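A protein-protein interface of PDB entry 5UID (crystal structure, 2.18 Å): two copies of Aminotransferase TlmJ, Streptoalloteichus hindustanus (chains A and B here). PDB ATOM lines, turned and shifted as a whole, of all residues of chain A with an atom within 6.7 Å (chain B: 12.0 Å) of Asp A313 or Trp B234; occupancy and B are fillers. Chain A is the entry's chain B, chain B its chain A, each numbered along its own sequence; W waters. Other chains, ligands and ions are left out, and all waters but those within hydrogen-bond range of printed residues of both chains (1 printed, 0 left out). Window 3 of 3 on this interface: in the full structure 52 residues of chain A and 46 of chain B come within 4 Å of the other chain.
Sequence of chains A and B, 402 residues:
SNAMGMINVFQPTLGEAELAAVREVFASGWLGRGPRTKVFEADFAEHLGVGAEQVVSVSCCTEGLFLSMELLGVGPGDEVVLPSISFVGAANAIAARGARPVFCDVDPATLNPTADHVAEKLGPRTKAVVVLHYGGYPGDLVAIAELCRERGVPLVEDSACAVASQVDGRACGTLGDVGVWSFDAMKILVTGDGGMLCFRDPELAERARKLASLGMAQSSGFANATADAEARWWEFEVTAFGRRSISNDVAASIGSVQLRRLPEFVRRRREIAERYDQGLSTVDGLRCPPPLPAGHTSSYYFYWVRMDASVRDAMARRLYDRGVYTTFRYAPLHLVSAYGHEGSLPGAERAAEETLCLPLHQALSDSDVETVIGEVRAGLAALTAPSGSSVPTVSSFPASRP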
ATOM      1  N   MET A 307     -26.935 -24.782 -32.767  1.00  0.00           N
ATOM      2  CA  MET A 307     -28.236 -24.388 -33.290  1.00  0.00           C
ATOM      3  C   MET A 307     -28.379 -22.873 -33.231  1.00  0.00           C
ATOM      4  O   MET A 307     -27.456 -22.181 -32.809  1.00  0.00           O
ATOM      5  CB  MET A 307     -29.357 -25.071 -32.503  1.00  0.00           C
ATOM      6  CG  MET A 307     -29.372 -24.728 -31.023  1.00  0.00           C
ATOM      7  SD  MET A 307     -30.353 -26.026 -29.940  1.00  0.00           S
ATOM      8  CE  MET A 307     -29.052 -27.473 -29.961  1.00  0.00           C
ATOM      9  N   ASP A 308     -29.525 -22.353 -33.660  1.00  0.00           N
ATOM     10  CA  ASP A 308     -29.749 -20.917 -33.595  1.00  0.00           C
ATOM     11  C   ASP A 308     -29.820 -20.460 -32.143  1.00  0.00           C
ATOM     12  O   ASP A 308     -30.380 -21.149 -31.284  1.00  0.00           O
ATOM     13  CB  ASP A 308     -31.033 -20.537 -34.329  1.00  0.00           C
ATOM     14  CG  ASP A 308     -31.250 -19.040 -34.377  1.00  0.00           C
ATOM     15  OD1 ASP A 308     -30.446 -18.344 -35.031  1.00  0.00           O
ATOM     16  OD2 ASP A 308     -32.219 -18.556 -33.759  1.00  0.00           O
ATOM     17  N   ALA A 309     -29.242 -19.287 -31.872  1.00  0.00           N
ATOM     18  CA  ALA A 309     -29.163 -18.791 -30.501  1.00  0.00           C
ATOM     19  C   ALA A 309     -30.542 -18.583 -29.887  1.00  0.00           C
ATOM     20  O   ALA A 309     -30.713 -18.757 -28.675  1.00  0.00           O
ATOM     21  CB  ALA A 309     -28.368 -17.486 -30.462  1.00  0.00           C
ATOM     22  N   SER A 310     -31.535 -18.219 -30.700  1.00  0.00           N
ATOM     23  CA  SER A 310     -32.869 -17.940 -30.183  1.00  0.00           C
ATOM     24  C   SER A 310     -33.606 -19.191 -29.724  1.00  0.00           C
ATOM     25  O   SER A 310     -34.681 -19.067 -29.129  1.00  0.00           O
ATOM     26  CB  SER A 310     -33.704 -17.222 -31.243  1.00  0.00           C
ATOM     27  OG  SER A 310     -33.993 -18.088 -32.328  1.00  0.00           O
ATOM     28  N   VAL A 311     -33.073 -20.381 -29.990  1.00  0.00           N
ATOM     29  CA  VAL A 311     -33.705 -21.623 -29.558  1.00  0.00           C
ATOM     30  C   VAL A 311     -32.812 -22.460 -28.655  1.00  0.00           C
ATOM     31  O   VAL A 311     -33.289 -23.470 -28.114  1.00  0.00           O
ATOM     32  CB  VAL A 311     -34.173 -22.471 -30.761  1.00  0.00           C
ATOM     33  CG1 VAL A 311     -34.955 -21.622 -31.745  1.00  0.00           C
ATOM     34  CG2 VAL A 311     -32.986 -23.140 -31.438  1.00  0.00           C
ATOM     35  N   ARG A 312     -31.544 -22.085 -28.467  1.00  0.00           N
ATOM     36  CA  ARG A 312     -30.638 -22.902 -27.663  1.00  0.00           C
ATOM     37  C   ARG A 312     -31.114 -22.987 -26.219  1.00  0.00           C
ATOM     38  O   ARG A 312     -31.180 -24.077 -25.639  1.00  0.00           O
ATOM     39  CB  ARG A 312     -29.216 -22.338 -27.734  1.00  0.00           C
ATOM     40  CG  ARG A 312     -28.106 -23.325 -27.340  1.00  0.00           C
ATOM     41  CD  ARG A 312     -27.908 -23.421 -25.826  1.00  0.00           C
ATOM     42  NE  ARG A 312     -27.796 -22.101 -25.210  1.00  0.00           N
ATOM     43  CZ  ARG A 312     -26.660 -21.420 -25.106  1.00  0.00           C
ATOM     44  NH1 ARG A 312     -26.651 -20.223 -24.534  1.00  0.00           N
ATOM     45  NH2 ARG A 312     -25.530 -21.934 -25.572  1.00  0.00           N
ATOM     46  N   ASP A 313     -31.446 -21.841 -25.618  1.00  0.00           N
ATOM     47  CA  ASP A 313     -31.908 -21.847 -24.235  1.00  0.00           C
ATOM     48  C   ASP A 313     -33.234 -22.584 -24.099  1.00  0.00           C
ATOM     49  O   ASP A 313     -33.420 -23.372 -23.164  1.00  0.00           O
ATOM     50  CB  ASP A 313     -32.032 -20.415 -23.712  1.00  0.00           C
ATOM     51  CG  ASP A 313     -30.688 -19.719 -23.592  1.00  0.00           C
ATOM     52  OD1 ASP A 313     -29.650 -20.414 -23.602  1.00  0.00           O
ATOM     53  OD2 ASP A 313     -30.670 -18.475 -23.478  1.00  0.00           O
ATOM     54  N   ALA A 314     -34.168 -22.344 -25.025  1.00  0.00           N
ATOM     55  CA  ALA A 314     -35.446 -23.050 -24.990  1.00  0.00           C
ATOM     56  C   ALA A 314     -35.260 -24.556 -25.135  1.00  0.00           C
ATOM     57  O   ALA A 314     -36.002 -25.332 -24.523  1.00  0.00           O
ATOM     58  CB  ALA A 314     -36.373 -22.519 -26.084  1.00  0.00           C
ATOM     59  N   MET A 315     -34.282 -24.983 -25.930  1.00  0.00           N
ATOM     60  CA  MET A 315     -33.977 -26.402 -26.087  1.00  0.00           C
ATOM     61  C   MET A 315     -33.538 -27.018 -24.765  1.00  0.00           C
ATOM     62  O   MET A 315     -34.005 -28.090 -24.385  1.00  0.00           O
ATOM     63  CB  MET A 315     -32.886 -26.609 -27.140  1.00  0.00           C
ATOM     64  CG  MET A 315     -32.492 -28.070 -27.354  1.00  0.00           C
ATOM     65  SD  MET A 315     -33.891 -29.113 -28.240  1.00  0.00           S
ATOM     66  CE  MET A 315     -34.159 -27.938 -29.769  1.00  0.00           C
ATOM     67  N   ALA A 316     -32.634 -26.327 -24.067  1.00  0.00           N
ATOM     68  CA  ALA A 316     -32.149 -26.832 -22.788  1.00  0.00           C
ATOM     69  C   ALA A 316     -33.285 -26.958 -21.781  1.00  0.00           C
ATOM     70  O   ALA A 316     -33.369 -27.953 -21.050  1.00  0.00           O
ATOM     71  CB  ALA A 316     -31.045 -25.922 -22.246  1.00  0.00           C
ATOM     72  N   ARG A 317     -34.174 -25.965 -21.733  1.00  0.00           N
ATOM     73  CA  ARG A 317     -35.295 -26.022 -20.800  1.00  0.00           C
ATOM     74  C   ARG A 317     -36.288 -27.109 -21.195  1.00  0.00           C
ATOM     75  O   ARG A 317     -36.808 -27.824 -20.330  1.00  0.00           O
ATOM     76  CB  ARG A 317     -35.988 -24.663 -20.721  1.00  0.00           C
ATOM     77  CG  ARG A 317     -37.114 -24.608 -19.698  1.00  0.00           C
ATOM     78  CD  ARG A 317     -36.611 -24.993 -18.315  1.00  0.00           C
ATOM     79  NE  ARG A 317     -37.678 -25.020 -17.319  1.00  0.00           N
ATOM     80  CZ  ARG A 317     -37.498 -25.356 -16.046  1.00  0.00           C
ATOM     81  NH1 ARG A 317     -36.290 -25.692 -15.613  1.00  0.00           N
ATOM     82  NH2 ARG A 317     -38.524 -25.356 -15.205  1.00  0.00           N
ATOM     83  N   ARG A 318     -36.568 -27.251 -22.493  1.00  0.00           N
ATOM     84  CA  ARG A 318     -37.482 -28.299 -22.935  1.00  0.00           C
ATOM     85  C   ARG A 318     -36.902 -29.683 -22.672  1.00  0.00           C
ATOM     86  O   ARG A 318     -37.625 -30.594 -22.249  1.00  0.00           O
ATOM     87  CB  ARG A 318     -37.806 -28.133 -24.417  1.00  0.00           C
ATOM     88  CG  ARG A 318     -38.739 -29.209 -24.959  1.00  0.00           C
ATOM     89  CD  ARG A 318     -38.862 -29.131 -26.469  1.00  0.00           C
ATOM     90  NE  ARG A 318     -39.555 -30.292 -27.022  1.00  0.00           N
ATOM     91  CZ  ARG A 318     -40.841 -30.310 -27.353  1.00  0.00           C
ATOM     92  NH1 ARG A 318     -41.584 -29.224 -27.190  1.00  0.00           N
ATOM     93  NH2 ARG A 318     -41.384 -31.412 -27.850  1.00  0.00           N
ATOM     94  N   THR A 326     -28.947 -31.171 -19.960  1.00  0.00           N
ATOM     95  CA  THR A 326     -27.932 -30.612 -20.841  1.00  0.00           C
ATOM     96  C   THR A 326     -27.319 -29.398 -20.160  1.00  0.00           C
ATOM     97  O   THR A 326     -27.858 -28.880 -19.180  1.00  0.00           O
ATOM     98  CB  THR A 326     -28.505 -30.210 -22.210  1.00  0.00           C
ATOM     99  OG1 THR A 326     -29.490 -29.185 -22.039  1.00  0.00           O
ATOM    100  CG2 THR A 326     -29.130 -31.406 -22.914  1.00  0.00           C
ATOM    101  N   THR A 327     -26.189 -28.941 -20.691  1.00  0.00           N
ATOM    102  CA  THR A 327     -25.515 -27.756 -20.170  1.00  0.00           C
ATOM    103  C   THR A 327     -24.569 -27.230 -21.244  1.00  0.00           C
ATOM    104  O   THR A 327     -24.549 -27.725 -22.377  1.00  0.00           O
ATOM    105  CB  THR A 327     -24.768 -28.067 -18.867  1.00  0.00           C
ATOM    106  OG1 THR A 327     -24.244 -26.851 -18.319  1.00  0.00           O
ATOM    107  CG2 THR A 327     -23.620 -29.033 -19.128  1.00  0.00           C
ATOM    108  N   PHE A 328     -23.783 -26.217 -20.888  1.00  0.00           N
ATOM    109  CA  PHE A 328     -22.773 -25.669 -21.777  1.00  0.00           C
ATOM    110  C   PHE A 328     -21.445 -25.557 -21.046  1.00  0.00           C
ATOM    111  O   PHE A 328     -21.397 -25.186 -19.868  1.00  0.00           O
ATOM    112  CB  PHE A 328     -23.174 -24.291 -22.321  1.00  0.00           C
ATOM    113  CG  PHE A 328     -22.067 -23.605 -23.074  1.00  0.00           C
ATOM    114  CD1 PHE A 328     -21.689 -24.049 -24.330  1.00  0.00           C
ATOM    115  CD2 PHE A 328     -21.390 -22.532 -22.516  1.00  0.00           C
ATOM    116  CE1 PHE A 328     -20.665 -23.432 -25.021  1.00  0.00           C
ATOM    117  CE2 PHE A 328     -20.366 -21.910 -23.202  1.00  0.00           C
ATOM    118  CZ  PHE A 328     -20.003 -22.361 -24.458  1.00  0.00           C
ATOM    119  N   ARG A 329     -20.374 -25.898 -21.754  1.00  0.00           N
ATOM    120  CA  ARG A 329     -19.006 -25.680 -21.312  1.00  0.00           C
ATOM    121  C   ARG A 329     -18.226 -25.146 -22.501  1.00  0.00           C
ATOM    122  O   ARG A 329     -18.480 -25.557 -23.635  1.00  0.00           O
ATOM    123  CB  ARG A 329     -18.358 -26.975 -20.797  1.00  0.00           C
ATOM    124  CG  ARG A 329     -19.047 -27.604 -19.597  1.00  0.00           C
ATOM    125  CD  ARG A 329     -18.774 -26.816 -18.328  1.00  0.00           C
ATOM    126  NE  ARG A 329     -19.272 -27.505 -17.142  1.00  0.00           N
ATOM    127  CZ  ARG A 329     -20.485 -27.328 -16.631  1.00  0.00           C
ATOM    128  NH1 ARG A 329     -21.328 -26.478 -17.201  1.00  0.00           N
ATOM    129  NH2 ARG A 329     -20.854 -27.997 -15.548  1.00  0.00           N
ATOM    130  N   TYR A 330     -17.310 -24.211 -22.262  1.00  0.00           N
ATOM    131  CA  TYR A 330     -17.107 -23.576 -20.965  1.00  0.00           C
ATOM    132  C   TYR A 330     -17.509 -22.113 -21.091  1.00  0.00           C
ATOM    133  O   TYR A 330     -17.277 -21.497 -22.133  1.00  0.00           O
ATOM    134  CB  TYR A 330     -15.649 -23.700 -20.511  1.00  0.00           C
ATOM    135  CG  TYR A 330     -15.184 -25.130 -20.333  1.00  0.00           C
ATOM    136  CD1 TYR A 330     -14.726 -25.875 -21.413  1.00  0.00           C
ATOM    137  CD2 TYR A 330     -15.206 -25.733 -19.083  1.00  0.00           C
ATOM    138  CE1 TYR A 330     -14.306 -27.183 -21.251  1.00  0.00           C
ATOM    139  CE2 TYR A 330     -14.786 -27.040 -18.911  1.00  0.00           C
ATOM    140  CZ  TYR A 330     -14.341 -27.759 -19.997  1.00  0.00           C
ATOM    141  OH  TYR A 330     -13.925 -29.056 -19.826  1.00  0.00           O
ATOM    142  N   ALA A 331     -18.115 -21.569 -20.039  1.00  0.00           N
ATOM    143  CA  ALA A 331     -18.621 -20.203 -20.087  1.00  0.00           C
ATOM    144  C   ALA A 331     -17.502 -19.237 -20.467  1.00  0.00           C
ATOM    145  O   ALA A 331     -16.415 -19.291 -19.875  1.00  0.00           O
ATOM    146  CB  ALA A 331     -19.225 -19.808 -18.740  1.00  0.00           C
ATOM    147  N   PRO A 332     -17.721 -18.350 -21.443  1.00  0.00           N
ATOM    148  CA  PRO A 332     -16.629 -17.493 -21.931  1.00  0.00           C
ATOM    149  C   PRO A 332     -16.080 -16.571 -20.855  1.00  0.00           C
ATOM    150  O   PRO A 332     -16.756 -15.640 -20.409  1.00  0.00           O
ATOM    151  CB  PRO A 332     -17.289 -16.704 -23.070  1.00  0.00           C
ATOM    152  CG  PRO A 332     -18.747 -16.724 -22.748  1.00  0.00           C
ATOM    153  CD  PRO A 332     -19.002 -18.052 -22.100  1.00  0.00           C
ATOM    154  N   ALA A 352     -20.904 -19.448 -27.279  1.00  0.00           N
ATOM    155  CA  ALA A 352     -21.593 -19.382 -25.996  1.00  0.00           C
ATOM    156  C   ALA A 352     -23.101 -19.235 -26.150  1.00  0.00           C
ATOM    157  O   ALA A 352     -23.838 -19.527 -25.204  1.00  0.00           O
ATOM    158  CB  ALA A 352     -21.043 -18.226 -25.160  1.00  0.00           C
ATOM    159  N   GLU A 353     -23.575 -18.791 -27.314  1.00  0.00           N
ATOM    160  CA  GLU A 353     -25.002 -18.633 -27.554  1.00  0.00           C
ATOM    161  C   GLU A 353     -25.619 -19.781 -28.339  1.00  0.00           C
ATOM    162  O   GLU A 353     -26.829 -20.004 -28.226  1.00  0.00           O
ATOM    163  CB  GLU A 353     -25.274 -17.327 -28.307  1.00  0.00           C
ATOM    164  CG  GLU A 353     -25.004 -16.070 -27.507  1.00  0.00           C
ATOM    165  CD  GLU A 353     -25.313 -14.814 -28.296  1.00  0.00           C
ATOM    166  OE1 GLU A 353     -25.528 -14.921 -29.522  1.00  0.00           O
ATOM    167  OE2 GLU A 353     -25.346 -13.722 -27.692  1.00  0.00           O
ATOM    168  N   THR A 355     -24.203 -23.185 -28.709  1.00  0.00           N
ATOM    169  CA  THR A 355     -23.742 -24.531 -28.409  1.00  0.00           C
ATOM    170  C   THR A 355     -24.491 -25.108 -27.215  1.00  0.00           C
ATOM    171  O   THR A 355     -24.733 -24.415 -26.222  1.00  0.00           O
ATOM    172  CB  THR A 355     -22.238 -24.537 -28.134  1.00  0.00           C
ATOM    173  OG1 THR A 355     -21.559 -23.858 -29.197  1.00  0.00           O
ATOM    174  CG2 THR A 355     -21.714 -25.965 -28.036  1.00  0.00           C
ATOM    175  N   LEU A 356     -24.859 -26.384 -27.322  1.00  0.00           N
ATOM    176  CA  LEU A 356     -25.445 -27.138 -26.226  1.00  0.00           C
ATOM    177  C   LEU A 356     -24.755 -28.492 -26.146  1.00  0.00           C
ATOM    178  O   LEU A 356     -24.500 -29.128 -27.172  1.00  0.00           O
ATOM    179  CB  LEU A 356     -26.958 -27.320 -26.409  1.00  0.00           C
ATOM    180  CG  LEU A 356     -27.724 -27.848 -25.195  1.00  0.00           C
ATOM    181  CD1 LEU A 356     -27.647 -26.862 -24.043  1.00  0.00           C
ATOM    182  CD2 LEU A 356     -29.174 -28.142 -25.549  1.00  0.00           C
ATOM    183  N   LEU A 383     -39.494 -26.105 -32.025  1.00  0.00           N
ATOM    184  CA  LEU A 383     -38.959 -24.753 -31.968  1.00  0.00           C
ATOM    185  C   LEU A 383     -38.593 -24.205 -33.343  1.00  0.00           C
ATOM    186  O   LEU A 383     -37.972 -23.143 -33.429  1.00  0.00           O
ATOM    187  CB  LEU A 383     -37.743 -24.715 -31.041  1.00  0.00           C
ATOM    188  CG  LEU A 383     -38.021 -25.137 -29.596  1.00  0.00           C
ATOM    189  CD1 LEU A 383     -36.728 -25.364 -28.828  1.00  0.00           C
ATOM    190  CD2 LEU A 383     -38.889 -24.101 -28.893  1.00  0.00           C
ATOM    191  N   SER B 213     -14.873 -22.797  -3.670  1.00  0.00           N
ATOM    192  CA  SER B 213     -15.404 -23.201  -4.972  1.00  0.00           C
ATOM    193  C   SER B 213     -14.981 -22.231  -6.068  1.00  0.00           C
ATOM    194  O   SER B 213     -15.813 -21.705  -6.809  1.00  0.00           O
ATOM    195  CB  SER B 213     -16.922 -23.319  -4.908  1.00  0.00           C
ATOM    196  OG  SER B 213     -17.317 -24.444  -4.143  1.00  0.00           O
ATOM    197  N   LEU B 214     -13.674 -21.979  -6.168  1.00  0.00           N
ATOM    198  CA  LEU B 214     -13.076 -21.182  -7.240  1.00  0.00           C
ATOM    199  C   LEU B 214     -13.537 -19.728  -7.223  1.00  0.00           C
ATOM    200  O   LEU B 214     -13.412 -19.023  -8.229  1.00  0.00           O
ATOM    201  CB  LEU B 214     -13.357 -21.805  -8.614  1.00  0.00           C
ATOM    202  CG  LEU B 214     -12.775 -23.198  -8.855  1.00  0.00           C
ATOM    203  CD1 LEU B 214     -13.658 -23.986  -9.803  1.00  0.00           C
ATOM    204  CD2 LEU B 214     -11.367 -23.091  -9.414  1.00  0.00           C
ATOM    205  N   GLY B 215     -14.062 -19.258  -6.093  1.00  0.00           N
ATOM    206  CA  GLY B 215     -14.577 -17.903  -6.022  1.00  0.00           C
ATOM    207  C   GLY B 215     -15.826 -17.649  -6.833  1.00  0.00           C
ATOM    208  O   GLY B 215     -16.195 -16.486  -7.025  1.00  0.00           O
ATOM    209  N   MET B 216     -16.490 -18.695  -7.316  1.00  0.00           N
ATOM    210  CA  MET B 216     -17.677 -18.540  -8.153  1.00  0.00           C
ATOM    211  C   MET B 216     -18.918 -18.152  -7.352  1.00  0.00           C
ATOM    212  O   MET B 216     -19.043 -18.486  -6.175  1.00  0.00           O
ATOM    213  CB  MET B 216     -17.957 -19.831  -8.926  1.00  0.00           C
ATOM    214  CG  MET B 216     -16.956 -20.138 -10.024  1.00  0.00           C
ATOM    215  SD  MET B 216     -17.464 -21.708 -11.072  1.00  0.00           S
ATOM    216  CE  MET B 216     -17.286 -23.071  -9.694  1.00  0.00           C
ATOM    217  N   ALA B 217     -19.835 -17.444  -8.011  1.00  0.00           N
ATOM    218  CA  ALA B 217     -21.120 -17.099  -7.423  1.00  0.00           C
ATOM    219  C   ALA B 217     -22.152 -16.986  -8.535  1.00  0.00           C
ATOM    220  O   ALA B 217     -21.814 -16.827  -9.711  1.00  0.00           O
ATOM    221  CB  ALA B 217     -21.045 -15.796  -6.618  1.00  0.00           C
ATOM    222  N   GLN B 218     -23.421 -17.074  -8.148  1.00  0.00           N
ATOM    223  CA  GLN B 218     -24.523 -16.990  -9.104  1.00  0.00           C
ATOM    224  C   GLN B 218     -24.762 -15.549  -9.543  1.00  0.00           C
ATOM    225  O   GLN B 218     -24.887 -14.647  -8.713  1.00  0.00           O
ATOM    226  CB  GLN B 218     -25.801 -17.576  -8.503  1.00  0.00           C
ATOM    227  N   ARG B 232     -27.701 -19.748 -19.263  1.00  0.00           N
ATOM    228  CA  ARG B 232     -28.682 -19.927 -18.200  1.00  0.00           C
ATOM    229  C   ARG B 232     -28.016 -20.367 -16.898  1.00  0.00           C
ATOM    230  O   ARG B 232     -27.367 -19.568 -16.225  1.00  0.00           O
ATOM    231  CB  ARG B 232     -29.746 -20.946 -18.618  1.00  0.00           C
ATOM    232  N   TRP B 233     -28.176 -21.645 -16.548  1.00  0.00           N
ATOM    233  CA  TRP B 233     -27.680 -22.145 -15.273  1.00  0.00           C
ATOM    234  C   TRP B 233     -26.191 -22.469 -15.286  1.00  0.00           C
ATOM    235  O   TRP B 233     -25.637 -22.789 -14.228  1.00  0.00           O
ATOM    236  CB  TRP B 233     -28.479 -23.381 -14.840  1.00  0.00           C
ATOM    237  CG  TRP B 233     -28.590 -24.461 -15.882  1.00  0.00           C
ATOM    238  CD1 TRP B 233     -27.635 -25.375 -16.221  1.00  0.00           C
ATOM    239  CD2 TRP B 233     -29.734 -24.756 -16.698  1.00  0.00           C
ATOM    240  NE1 TRP B 233     -28.108 -26.212 -17.206  1.00  0.00           N
ATOM    241  CE2 TRP B 233     -29.392 -25.853 -17.515  1.00  0.00           C
ATOM    242  CE3 TRP B 233     -31.009 -24.194 -16.821  1.00  0.00           C
ATOM    243  CZ2 TRP B 233     -30.279 -26.398 -18.442  1.00  0.00           C
ATOM    244  CZ3 TRP B 233     -31.888 -24.738 -17.743  1.00  0.00           C
ATOM    245  CH2 TRP B 233     -31.519 -25.829 -18.541  1.00  0.00           C
ATOM    246  N   TRP B 234     -25.528 -22.382 -16.438  1.00  0.00           N
ATOM    247  CA  TRP B 234     -24.100 -22.661 -16.519  1.00  0.00           C
ATOM    248  C   TRP B 234     -23.236 -21.412 -16.401  1.00  0.00           C
ATOM    249  O   TRP B 234     -22.010 -21.536 -16.297  1.00  0.00           O
ATOM    250  CB  TRP B 234     -23.774 -23.380 -17.833  1.00  0.00           C
ATOM    251  CG  TRP B 234     -24.313 -22.692 -19.047  1.00  0.00           C
ATOM    252  CD1 TRP B 234     -23.755 -21.637 -19.707  1.00  0.00           C
ATOM    253  CD2 TRP B 234     -25.519 -23.016 -19.752  1.00  0.00           C
ATOM    254  NE1 TRP B 234     -24.540 -21.280 -20.777  1.00  0.00           N
ATOM    255  CE2 TRP B 234     -25.628 -22.112 -20.828  1.00  0.00           C
ATOM    256  CE3 TRP B 234     -26.518 -23.980 -19.577  1.00  0.00           C
ATOM    257  CZ2 TRP B 234     -26.695 -22.142 -21.722  1.00  0.00           C
ATOM    258  CZ3 TRP B 234     -27.576 -24.010 -20.469  1.00  0.00           C
ATOM    259  CH2 TRP B 234     -27.656 -23.097 -21.528  1.00  0.00           C
ATOM    260  N   GLU B 235     -23.832 -20.224 -16.412  1.00  0.00           N
ATOM    261  CA  GLU B 235     -23.070 -18.987 -16.343  1.00  0.00           C
ATOM    262  C   GLU B 235     -22.849 -18.583 -14.890  1.00  0.00           C
ATOM    263  O   GLU B 235     -23.655 -18.894 -14.009  1.00  0.00           O
ATOM    264  CB  GLU B 235     -23.785 -17.873 -17.107  1.00  0.00           C
ATOM    265  CG  GLU B 235     -22.847 -16.831 -17.690  1.00  0.00           C
ATOM    266  CD  GLU B 235     -23.479 -16.047 -18.824  1.00  0.00           C
ATOM    267  OE1 GLU B 235     -24.675 -16.271 -19.112  1.00  0.00           O
ATOM    268  OE2 GLU B 235     -22.777 -15.209 -19.430  1.00  0.00           O
ATOM    269  N   PHE B 236     -21.741 -17.887 -14.646  1.00  0.00           N
ATOM    270  CA  PHE B 236     -21.322 -17.578 -13.287  1.00  0.00           C
ATOM    271  C   PHE B 236     -20.529 -16.279 -13.277  1.00  0.00           C
ATOM    272  O   PHE B 236     -20.119 -15.765 -14.321  1.00  0.00           O
ATOM    273  CB  PHE B 236     -20.481 -18.717 -12.697  1.00  0.00           C
ATOM    274  CG  PHE B 236     -19.281 -19.071 -13.528  1.00  0.00           C
ATOM    275  CD1 PHE B 236     -18.070 -18.428 -13.332  1.00  0.00           C
ATOM    276  CD2 PHE B 236     -19.367 -20.038 -14.515  1.00  0.00           C
ATOM    277  CE1 PHE B 236     -16.966 -18.749 -14.105  1.00  0.00           C
ATOM    278  CE2 PHE B 236     -18.267 -20.364 -15.288  1.00  0.00           C
ATOM    279  CZ  PHE B 236     -17.066 -19.718 -15.082  1.00  0.00           C
ATOM    280  N   GLU B 237     -20.311 -15.757 -12.071  1.00  0.00           N
ATOM    281  CA  GLU B 237     -19.437 -14.619 -11.836  1.00  0.00           C
ATOM    282  C   GLU B 237     -18.323 -15.031 -10.879  1.00  0.00           C
ATOM    283  O   GLU B 237     -18.460 -15.985 -10.109  1.00  0.00           O
ATOM    284  CB  GLU B 237     -20.212 -13.424 -11.263  1.00  0.00           C
ATOM    285  N   VAL B 238     -17.214 -14.301 -10.936  1.00  0.00           N
ATOM    286  CA  VAL B 238     -16.030 -14.592 -10.133  1.00  0.00           C
ATOM    287  C   VAL B 238     -15.815 -13.436  -9.165  1.00  0.00           C
ATOM    288  O   VAL B 238     -15.604 -12.293  -9.587  1.00  0.00           O
ATOM    289  CB  VAL B 238     -14.791 -14.817 -11.013  1.00  0.00           C
ATOM    290  CG1 VAL B 238     -13.555 -15.005 -10.150  1.00  0.00           C
ATOM    291  CG2 VAL B 238     -14.998 -16.023 -11.927  1.00  0.00           C
HETATM  292  O   HOH W   1     -19.778 -16.042 -19.379  1.00  0.00           O
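Among the printed residues, pairs that only touch across the chains: Arg A312 with Trp B234, Thr A327 with Trp B234, Phe A328 with Trp B234, Ala A331 with Phe B236, Ala A316 with Trp B233, Asp A313 with Trp B234 and Arg A329 with Trp B234.
Water W1 lies within hydrogen-bond range of the side-chain carboxylate (OE2) of Glu B235 and the backbone carbonyl oxygen (O) of Pro A332.
Hydrophobic or aromatic side chains of chain A that line the printed part of chain B: Ala A316, Phe A328 and Ala A331.
Of the 13 printed residues of chain B, 3 touch a printed residue of chain A.
Hydrophobic or aromatic side chains of chain B within 4 Å of the printed part of chain A: Trp B233, Trp B234 and Phe B236.
No residue of chain B comes within 4 Å of Ala A309.
No residue of chain B comes within 4 Å of Val A311.
Asp A313 touches just one residue of chain B: Trp B234 (3.9 Å).
No residue of chain B comes within 4 Å of Met A315.
Of chain B, only Trp B233 (3.3 Å) comes within 4 Å of Thr A326.
Of the printed residues of chain B, Thr A327 touches Trp B234 (3.5 Å).
Of chain B, only Trp B234 comes within 4 Å of Phe A328.
Of the printed residues of chain B, Arg A329 touches Trp B234.
Ala A331 touches just one residue of chain B: Phe B236.
Pro A332 touches none of the printed residues of chain B.
Printed residues of chain A within 4 Å of Trp B233: Ala A316 and Thr A326.
Of the printed residues of chain A, Trp B234 touches Arg A312, Asp A313, Thr A327, Phe A328 and Arg A329.
Printed residues of chain A within 4 Å of Phe B236: Ala A331 (3.6 Å).
Val B238 touches none of the printed residues of chain A.
The nearest residue of chain B that does not touch Asp A313 is Arg B232 (4.8 Å).
The indole nitrogen (NE1) of Trp B233 sits at hydrogen-bond distance from the backbone carbonyl oxygen (O) of Thr A326, 3.3 Å away.
No position is printed for both chains.
The guanidinium group (NE) of Arg A312 is in salt-bridge range of the side-chain carboxylate (OD1) of Asp A313, at 3.0 Å.
The backbone carbonyl oxygen (O) of Ala A352 is in hydrogen-bond range of the guanidinium group (NH2) of Arg A312 (3.0 Å).
NH2 of Arg A312 lies within hydrogen-bond range of O of Thr A355, 2.7 Å away.
The side-chain hydroxyl (OG1) of Thr A327 is in hydrogen-bond range of the guanidinium group (NH1) of Arg A329 (3.1 Å).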
